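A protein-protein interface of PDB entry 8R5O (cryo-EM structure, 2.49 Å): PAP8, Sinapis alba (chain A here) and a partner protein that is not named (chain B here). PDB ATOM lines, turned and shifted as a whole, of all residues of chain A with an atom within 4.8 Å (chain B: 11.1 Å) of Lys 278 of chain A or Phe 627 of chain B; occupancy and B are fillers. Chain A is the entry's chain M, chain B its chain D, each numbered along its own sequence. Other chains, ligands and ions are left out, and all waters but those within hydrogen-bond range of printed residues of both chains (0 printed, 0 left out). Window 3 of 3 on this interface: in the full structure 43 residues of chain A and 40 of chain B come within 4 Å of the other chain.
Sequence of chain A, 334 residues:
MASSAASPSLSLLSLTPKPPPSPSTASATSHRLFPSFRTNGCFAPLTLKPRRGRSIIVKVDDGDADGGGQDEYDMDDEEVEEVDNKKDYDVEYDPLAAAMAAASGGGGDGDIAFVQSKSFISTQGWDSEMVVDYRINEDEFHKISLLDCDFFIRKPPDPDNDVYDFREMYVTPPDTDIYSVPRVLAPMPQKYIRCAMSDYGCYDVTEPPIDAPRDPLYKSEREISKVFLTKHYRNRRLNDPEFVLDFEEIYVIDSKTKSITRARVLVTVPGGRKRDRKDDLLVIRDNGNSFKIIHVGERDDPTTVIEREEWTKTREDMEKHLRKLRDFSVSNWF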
ATOM      1  N   PRO A 241      -4.384 -11.111  20.847  1.00  0.00           N
ATOM      2  CA  PRO A 241      -3.890 -11.046  22.233  1.00  0.00           C
ATOM      3  C   PRO A 241      -4.928 -11.435  23.273  1.00  0.00           C
ATOM      4  O   PRO A 241      -4.550 -11.757  24.406  1.00  0.00           O
ATOM      5  CB  PRO A 241      -3.465  -9.580  22.387  1.00  0.00           C
ATOM      6  CG  PRO A 241      -4.239  -8.847  21.341  1.00  0.00           C
ATOM      7  CD  PRO A 241      -4.354  -9.795  20.186  1.00  0.00           C
ATOM      8  N   PHE A 243      -6.984 -14.055  22.810  1.00  0.00           N
ATOM      9  CA  PHE A 243      -7.416 -15.391  22.425  1.00  0.00           C
ATOM     10  C   PHE A 243      -7.531 -16.295  23.644  1.00  0.00           C
ATOM     11  O   PHE A 243      -6.595 -16.408  24.441  1.00  0.00           O
ATOM     12  CB  PHE A 243      -6.439 -15.999  21.420  1.00  0.00           C
ATOM     13  CG  PHE A 243      -6.585 -17.487  21.262  1.00  0.00           C
ATOM     14  CD1 PHE A 243      -7.600 -18.018  20.487  1.00  0.00           C
ATOM     15  CD2 PHE A 243      -5.707 -18.354  21.894  1.00  0.00           C
ATOM     16  CE1 PHE A 243      -7.738 -19.385  20.345  1.00  0.00           C
ATOM     17  CE2 PHE A 243      -5.841 -19.720  21.756  1.00  0.00           C
ATOM     18  CZ  PHE A 243      -6.857 -20.236  20.981  1.00  0.00           C
ATOM     19  N   VAL A 244      -8.687 -16.944  23.779  1.00  0.00           N
ATOM     20  CA  VAL A 244      -8.897 -18.016  24.740  1.00  0.00           C
ATOM     21  C   VAL A 244      -9.793 -19.059  24.089  1.00  0.00           C
ATOM     22  O   VAL A 244     -10.508 -18.781  23.125  1.00  0.00           O
ATOM     23  CB  VAL A 244      -9.526 -17.527  26.066  1.00  0.00           C
ATOM     24  CG1 VAL A 244      -8.473 -16.899  26.962  1.00  0.00           C
ATOM     25  CG2 VAL A 244     -10.651 -16.549  25.791  1.00  0.00           C
ATOM     26  N   ASP A 276     -13.810 -15.288  34.072  1.00  0.00           N
ATOM     27  CA  ASP A 276     -12.513 -15.149  33.421  1.00  0.00           C
ATOM     28  C   ASP A 276     -12.141 -16.492  32.808  1.00  0.00           C
ATOM     29  O   ASP A 276     -11.745 -17.423  33.512  1.00  0.00           O
ATOM     30  CB  ASP A 276     -11.459 -14.681  34.418  1.00  0.00           C
ATOM     31  CG  ASP A 276     -10.159 -14.287  33.748  1.00  0.00           C
ATOM     32  OD1 ASP A 276     -10.167 -14.053  32.522  1.00  0.00           O
ATOM     33  OD2 ASP A 276      -9.125 -14.214  34.447  1.00  0.00           O
ATOM     34  N   ARG A 277     -12.270 -16.596  31.485  1.00  0.00           N
ATOM     35  CA  ARG A 277     -11.941 -17.829  30.783  1.00  0.00           C
ATOM     36  C   ARG A 277     -10.451 -18.138  30.807  1.00  0.00           C
ATOM     37  O   ARG A 277     -10.061 -19.243  30.425  1.00  0.00           O
ATOM     38  CB  ARG A 277     -12.424 -17.752  29.335  1.00  0.00           C
ATOM     39  CG  ARG A 277     -13.904 -17.448  29.187  1.00  0.00           C
ATOM     40  CD  ARG A 277     -14.738 -18.714  29.147  1.00  0.00           C
ATOM     41  NE  ARG A 277     -16.131 -18.430  28.829  1.00  0.00           N
ATOM     42  CZ  ARG A 277     -17.011 -19.340  28.436  1.00  0.00           C
ATOM     43  NH1 ARG A 277     -16.673 -20.612  28.299  1.00  0.00           N
ATOM     44  NH2 ARG A 277     -18.258 -18.965  28.171  1.00  0.00           N
ATOM     45  N   LYS A 278      -9.614 -17.190  31.227  1.00  0.00           N
ATOM     46  CA  LYS A 278      -8.181 -17.428  31.316  1.00  0.00           C
ATOM     47  C   LYS A 278      -7.801 -18.289  32.513  1.00  0.00           C
ATOM     48  O   LYS A 278      -6.651 -18.734  32.592  1.00  0.00           O
ATOM     49  CB  LYS A 278      -7.445 -16.090  31.376  1.00  0.00           C
ATOM     50  CG  LYS A 278      -7.958 -15.072  30.366  1.00  0.00           C
ATOM     51  CD  LYS A 278      -7.308 -13.711  30.557  1.00  0.00           C
ATOM     52  CE  LYS A 278      -6.013 -13.594  29.772  1.00  0.00           C
ATOM     53  NZ  LYS A 278      -6.259 -13.556  28.302  1.00  0.00           N
ATOM     54  N   ASP A 279      -8.729 -18.536  33.437  1.00  0.00           N
ATOM     55  CA  ASP A 279      -8.441 -19.275  34.657  1.00  0.00           C
ATOM     56  C   ASP A 279      -8.928 -20.718  34.638  1.00  0.00           C
ATOM     57  O   ASP A 279      -8.636 -21.458  35.581  1.00  0.00           O
ATOM     58  CB  ASP A 279      -9.064 -18.566  35.868  1.00  0.00           C
ATOM     59  CG  ASP A 279      -8.220 -17.415  36.369  1.00  0.00           C
ATOM     60  OD1 ASP A 279      -7.100 -17.226  35.854  1.00  0.00           O
ATOM     61  OD2 ASP A 279      -8.680 -16.698  37.283  1.00  0.00           O
ATOM     62  N   ASP A 280      -9.654 -21.143  33.611  1.00  0.00           N
ATOM     63  CA  ASP A 280     -10.283 -22.453  33.657  1.00  0.00           C
ATOM     64  C   ASP A 280      -9.458 -23.496  32.910  1.00  0.00           C
ATOM     65  O   ASP A 280      -8.752 -23.195  31.946  1.00  0.00           O
ATOM     66  CB  ASP A 280     -11.718 -22.404  33.117  1.00  0.00           C
ATOM     67  CG  ASP A 280     -11.817 -21.840  31.714  1.00  0.00           C
ATOM     68  OD1 ASP A 280     -10.792 -21.754  31.012  1.00  0.00           O
ATOM     69  OD2 ASP A 280     -12.941 -21.479  31.311  1.00  0.00           O
ATOM     70  N   HIS B 623      -5.180 -32.603  30.509  1.00  0.00           N
ATOM     71  CA  HIS B 623      -5.324 -31.288  31.121  1.00  0.00           C
ATOM     72  C   HIS B 623      -5.156 -30.245  30.026  1.00  0.00           C
ATOM     73  O   HIS B 623      -4.066 -30.088  29.471  1.00  0.00           O
ATOM     74  CB  HIS B 623      -4.309 -31.093  32.244  1.00  0.00           C
ATOM     75  CG  HIS B 623      -4.526 -32.000  33.414  1.00  0.00           C
ATOM     76  ND1 HIS B 623      -3.622 -32.114  34.448  1.00  0.00           N
ATOM     77  CD2 HIS B 623      -5.546 -32.836  33.714  1.00  0.00           C
ATOM     78  CE1 HIS B 623      -4.075 -32.983  35.333  1.00  0.00           C
ATOM     79  NE2 HIS B 623      -5.241 -33.436  34.911  1.00  0.00           N
ATOM     80  N   TYR B 624      -6.232 -29.527  29.729  1.00  0.00           N
ATOM     81  CA  TYR B 624      -6.323 -28.661  28.560  1.00  0.00           C
ATOM     82  C   TYR B 624      -6.451 -27.218  29.032  1.00  0.00           C
ATOM     83  O   TYR B 624      -7.508 -26.814  29.526  1.00  0.00           O
ATOM     84  CB  TYR B 624      -7.514 -29.077  27.701  1.00  0.00           C
ATOM     85  CG  TYR B 624      -7.418 -28.741  26.235  1.00  0.00           C
ATOM     86  CD1 TYR B 624      -6.682 -27.654  25.791  1.00  0.00           C
ATOM     87  CD2 TYR B 624      -8.074 -29.513  25.291  1.00  0.00           C
ATOM     88  CE1 TYR B 624      -6.602 -27.349  24.450  1.00  0.00           C
ATOM     89  CE2 TYR B 624      -8.003 -29.217  23.952  1.00  0.00           C
ATOM     90  CZ  TYR B 624      -7.267 -28.133  23.534  1.00  0.00           C
ATOM     91  OH  TYR B 624      -7.198 -27.840  22.195  1.00  0.00           O
ATOM     92  N   GLU B 625      -5.381 -26.444  28.880  1.00  0.00           N
ATOM     93  CA  GLU B 625      -5.403 -25.038  29.259  1.00  0.00           C
ATOM     94  C   GLU B 625      -6.129 -24.209  28.207  1.00  0.00           C
ATOM     95  O   GLU B 625      -6.094 -24.511  27.011  1.00  0.00           O
ATOM     96  CB  GLU B 625      -3.982 -24.507  29.447  1.00  0.00           C
ATOM     97  CG  GLU B 625      -3.173 -25.258  30.485  1.00  0.00           C
ATOM     98  CD  GLU B 625      -1.782 -24.686  30.657  1.00  0.00           C
ATOM     99  OE1 GLU B 625      -1.537 -23.562  30.174  1.00  0.00           O
ATOM    100  OE2 GLU B 625      -0.930 -25.363  31.271  1.00  0.00           O
ATOM    101  N   SER B 626      -6.790 -23.144  28.666  1.00  0.00           N
ATOM    102  CA  SER B 626      -7.566 -22.297  27.768  1.00  0.00           C
ATOM    103  C   SER B 626      -6.699 -21.468  26.832  1.00  0.00           C
ATOM    104  O   SER B 626      -7.234 -20.860  25.901  1.00  0.00           O
ATOM    105  CB  SER B 626      -8.485 -21.375  28.570  1.00  0.00           C
ATOM    106  OG  SER B 626      -7.742 -20.479  29.377  1.00  0.00           O
ATOM    107  N   PHE B 627      -5.388 -21.423  27.051  1.00  0.00           N
ATOM    108  CA  PHE B 627      -4.495 -20.711  26.152  1.00  0.00           C
ATOM    109  C   PHE B 627      -3.980 -21.577  25.010  1.00  0.00           C
ATOM    110  O   PHE B 627      -3.292 -21.060  24.126  1.00  0.00           O
ATOM    111  CB  PHE B 627      -3.312 -20.127  26.929  1.00  0.00           C
ATOM    112  CG  PHE B 627      -3.710 -19.104  27.953  1.00  0.00           C
ATOM    113  CD1 PHE B 627      -4.233 -17.883  27.563  1.00  0.00           C
ATOM    114  CD2 PHE B 627      -3.556 -19.361  29.306  1.00  0.00           C
ATOM    115  CE1 PHE B 627      -4.599 -16.941  28.501  1.00  0.00           C
ATOM    116  CE2 PHE B 627      -3.920 -18.421  30.247  1.00  0.00           C
ATOM    117  CZ  PHE B 627      -4.441 -17.210  29.845  1.00  0.00           C
ATOM    118  N   GLY B 628      -4.295 -22.869  25.001  1.00  0.00           N
ATOM    119  CA  GLY B 628      -3.975 -23.739  23.883  1.00  0.00           C
ATOM    120  C   GLY B 628      -3.084 -24.922  24.201  1.00  0.00           C
ATOM    121  O   GLY B 628      -3.059 -25.878  23.413  1.00  0.00           O
ATOM    122  N   ASN B 629      -2.347 -24.917  25.304  1.00  0.00           N
ATOM    123  CA  ASN B 629      -1.490 -26.042  25.653  1.00  0.00           C
ATOM    124  C   ASN B 629      -2.288 -27.105  26.395  1.00  0.00           C
ATOM    125  O   ASN B 629      -3.133 -26.789  27.235  1.00  0.00           O
ATOM    126  CB  ASN B 629      -0.312 -25.579  26.510  1.00  0.00           C
ATOM    127  CG  ASN B 629       0.754 -24.875  25.698  1.00  0.00           C
ATOM    128  OD1 ASN B 629       0.637 -23.690  25.394  1.00  0.00           O
ATOM    129  ND2 ASN B 629       1.805 -25.605  25.344  1.00  0.00           N
ATOM    130  N   TYR B 630      -2.025 -28.370  26.072  1.00  0.00           N
ATOM    131  CA  TYR B 630      -2.673 -29.474  26.764  1.00  0.00           C
ATOM    132  C   TYR B 630      -1.653 -30.553  27.097  1.00  0.00           C
ATOM    133  O   TYR B 630      -0.742 -30.826  26.313  1.00  0.00           O
ATOM    134  CB  TYR B 630      -3.839 -30.059  25.946  1.00  0.00           C
ATOM    135  CG  TYR B 630      -3.510 -30.501  24.538  1.00  0.00           C
ATOM    136  CD1 TYR B 630      -3.415 -29.582  23.502  1.00  0.00           C
ATOM    137  CD2 TYR B 630      -3.333 -31.844  24.235  1.00  0.00           C
ATOM    138  CE1 TYR B 630      -3.129 -29.985  22.213  1.00  0.00           C
ATOM    139  CE2 TYR B 630      -3.049 -32.256  22.950  1.00  0.00           C
ATOM    140  CZ  TYR B 630      -2.948 -31.323  21.943  1.00  0.00           C
ATOM    141  OH  TYR B 630      -2.665 -31.730  20.661  1.00  0.00           O
ATOM    142  N   HIS B 631      -1.816 -31.155  28.273  1.00  0.00           N
ATOM    143  CA  HIS B 631      -0.937 -32.204  28.775  1.00  0.00           C
ATOM    144  C   HIS B 631      -1.680 -33.530  28.719  1.00  0.00           C
ATOM    145  O   HIS B 631      -2.783 -33.649  29.260  1.00  0.00           O
ATOM    146  CB  HIS B 631      -0.491 -31.920  30.209  1.00  0.00           C
ATOM    147  CG  HIS B 631       0.401 -30.728  30.350  1.00  0.00           C
ATOM    148  ND1 HIS B 631       0.565 -29.794  29.349  1.00  0.00           N
ATOM    149  CD2 HIS B 631       1.182 -30.318  31.377  1.00  0.00           C
ATOM    150  CE1 HIS B 631       1.405 -28.860  29.756  1.00  0.00           C
ATOM    151  NE2 HIS B 631       1.796 -29.156  30.981  1.00  0.00           N
ATOM    152  N   VAL B 640       3.375 -33.218  26.186  1.00  0.00           N
ATOM    153  CA  VAL B 640       2.923 -31.834  26.203  1.00  0.00           C
ATOM    154  C   VAL B 640       2.836 -31.353  24.764  1.00  0.00           C
ATOM    155  O   VAL B 640       3.827 -31.396  24.027  1.00  0.00           O
ATOM    156  CB  VAL B 640       3.860 -30.944  27.031  1.00  0.00           C
ATOM    157  CG1 VAL B 640       3.385 -29.501  26.989  1.00  0.00           C
ATOM    158  CG2 VAL B 640       3.939 -31.445  28.463  1.00  0.00           C
ATOM    159  N   ARG B 641       1.652 -30.899  24.364  1.00  0.00           N
ATOM    160  CA  ARG B 641       1.393 -30.422  23.013  1.00  0.00           C
ATOM    161  C   ARG B 641       0.631 -29.104  23.090  1.00  0.00           C
ATOM    162  O   ARG B 641       0.238 -28.648  24.166  1.00  0.00           O
ATOM    163  CB  ARG B 641       0.614 -31.459  22.194  1.00  0.00           C
ATOM    164  CG  ARG B 641       1.409 -32.712  21.858  1.00  0.00           C
ATOM    165  CD  ARG B 641       0.709 -33.552  20.806  1.00  0.00           C
ATOM    166  NE  ARG B 641      -0.505 -34.180  21.312  1.00  0.00           N
ATOM    167  CZ  ARG B 641      -1.448 -34.708  20.545  1.00  0.00           C
ATOM    168  NH1 ARG B 641      -1.363 -34.675  19.226  1.00  0.00           N
ATOM    169  NH2 ARG B 641      -2.503 -35.281  21.115  1.00  0.00           N
ATOM    170  N   SER B 642       0.425 -28.487  21.930  1.00  0.00           N
ATOM    171  CA  SER B 642      -0.257 -27.204  21.864  1.00  0.00           C
ATOM    172  C   SER B 642      -1.028 -27.115  20.556  1.00  0.00           C
ATOM    173  O   SER B 642      -0.702 -27.784  19.573  1.00  0.00           O
ATOM    174  CB  SER B 642       0.730 -26.039  21.982  1.00  0.00           C
ATOM    175  OG  SER B 642       0.062 -24.792  21.939  1.00  0.00           O
ATOM    176  N   VAL B 643      -2.067 -26.276  20.557  1.00  0.00           N
ATOM    177  CA  VAL B 643      -2.787 -25.975  19.321  1.00  0.00           C
ATOM    178  C   VAL B 643      -2.266 -24.719  18.644  1.00  0.00           C
ATOM    179  O   VAL B 643      -2.725 -24.386  17.540  1.00  0.00           O
ATOM    180  CB  VAL B 643      -4.302 -25.826  19.566  1.00  0.00           C
ATOM    181  CG1 VAL B 643      -4.858 -27.080  20.212  1.00  0.00           C
ATOM    182  CG2 VAL B 643      -4.586 -24.601  20.415  1.00  0.00           C
ATOM    183  N   LYS B 644      -1.328 -24.007  19.264  1.00  0.00           N
ATOM    184  CA  LYS B 644      -0.718 -22.823  18.677  1.00  0.00           C
ATOM    185  C   LYS B 644       0.657 -23.113  18.086  1.00  0.00           C
ATOM    186  O   LYS B 644       0.957 -22.670  16.973  1.00  0.00           O
ATOM    187  CB  LYS B 644      -0.614 -21.707  19.724  1.00  0.00           C
ATOM    188  CG  LYS B 644      -1.955 -21.218  20.245  1.00  0.00           C
ATOM    189  CD  LYS B 644      -1.783 -20.177  21.341  1.00  0.00           C
ATOM    190  CE  LYS B 644      -1.102 -18.924  20.821  1.00  0.00           C
ATOM    191  NZ  LYS B 644      -1.896 -18.255  19.756  1.00  0.00           N
ATOM    192  N   LYS B 645       1.494 -23.853  18.804  1.00  0.00           N
ATOM    193  CA  LYS B 645       2.828 -24.203  18.342  1.00  0.00           C
ATOM    194  C   LYS B 645       2.879 -25.661  17.893  1.00  0.00           C
ATOM    195  O   LYS B 645       1.930 -26.427  18.063  1.00  0.00           O
ATOM    196  CB  LYS B 645       3.863 -23.951  19.444  1.00  0.00           C
ATOM    197  CG  LYS B 645       3.921 -22.516  19.935  1.00  0.00           C
ATOM    198  CD  LYS B 645       3.225 -22.355  21.276  1.00  0.00           C
ATOM    199  CE  LYS B 645       3.965 -23.107  22.371  1.00  0.00           C
ATOM    200  NZ  LYS B 645       3.340 -22.901  23.707  1.00  0.00           N
ATOM    201  N   THR B 647       5.119 -27.671  19.192  1.00  0.00           N
ATOM    202  CA  THR B 647       5.905 -28.309  20.238  1.00  0.00           C
ATOM    203  C   THR B 647       5.357 -29.694  20.566  1.00  0.00           C
ATOM    204  O   THR B 647       4.157 -29.957  20.458  1.00  0.00           O
ATOM    205  CB  THR B 647       5.919 -27.446  21.501  1.00  0.00           C
ATOM    206  OG1 THR B 647       4.586 -27.325  22.015  1.00  0.00           O
ATOM    207  CG2 THR B 647       6.469 -26.061  21.198  1.00  0.00           C
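The side-chain hydroxyl (OG) of Ser 626 of chain B is in hydrogen-bond range of the backbone carbonyl oxygen (O) of Arg 277 of chain A (2.8 Å).
OD1 of Asp 276 of chain A sits close to N of Lys 278 of chain A (3.4 Å). The backbone carbonyl oxygen of Arg 277 of chain A sits close to the side-chain carboxylate of Asp 280 of chain A (2.7 Å).
Among the printed residues, pairs that only touch across the chains: Phe 243 of chain A with Phe 627 of chain B (3.7 Å), Val 244 of chain A with Ser 626 of chain B (3.5 Å), Lys 278 of chain A with Ser 626 of chain B (3.6 Å), Lys 278 of chain A with Phe 627 of chain B (3.6 Å) and Asp 280 of chain A with Ser 626 of chain B (3.4 Å).
Of chain B, only Ser 626 and Phe 627 come within 4 Å of Lys 278 of chain A. Phe 627 of chain B touches just these residues of chain A: Phe 243 (3.7 Å) and Lys 278 (3.6 Å). Phe 243 of chain A touches one residue of chain B. Val 244 of chain A touches one residue of chain B. No residue of chain B comes within 4 Å of Asp 276 of chain A. No residue of chain B comes within 4 Å of Asp 279 of chain A. Of chain B, only Ser 626 (3.4 Å) comes within 4 Å of Asp 280 of chain A. Of the printed residues of chain A, Ser 626 of chain B touches Val 244, Arg 277, Lys 278 and Asp 280. Of the printed residues of chain B, Arg 277 of chain A touches Ser 626 (2.8 Å). The nearest residue of chain B that does not touch Lys 278 of chain A is Glu 625 of chain B (7.0 Å). The nearest residue of chain A that does not touch Phe 627 of chain B is Val 244 of chain A (4.2 Å).
Hydrophobic or aromatic side chains of chain A that line the printed part of chain B: Phe 243. Of the 16 printed residues of chain B, 2 touch a printed residue of chain A. Among the printed residues, 6 pairs touch across the chains. Among the printed residues, no Asp or Glu carboxylate lies within 4 Å of a Lys or Arg side-chain nitrogen of the other chain.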
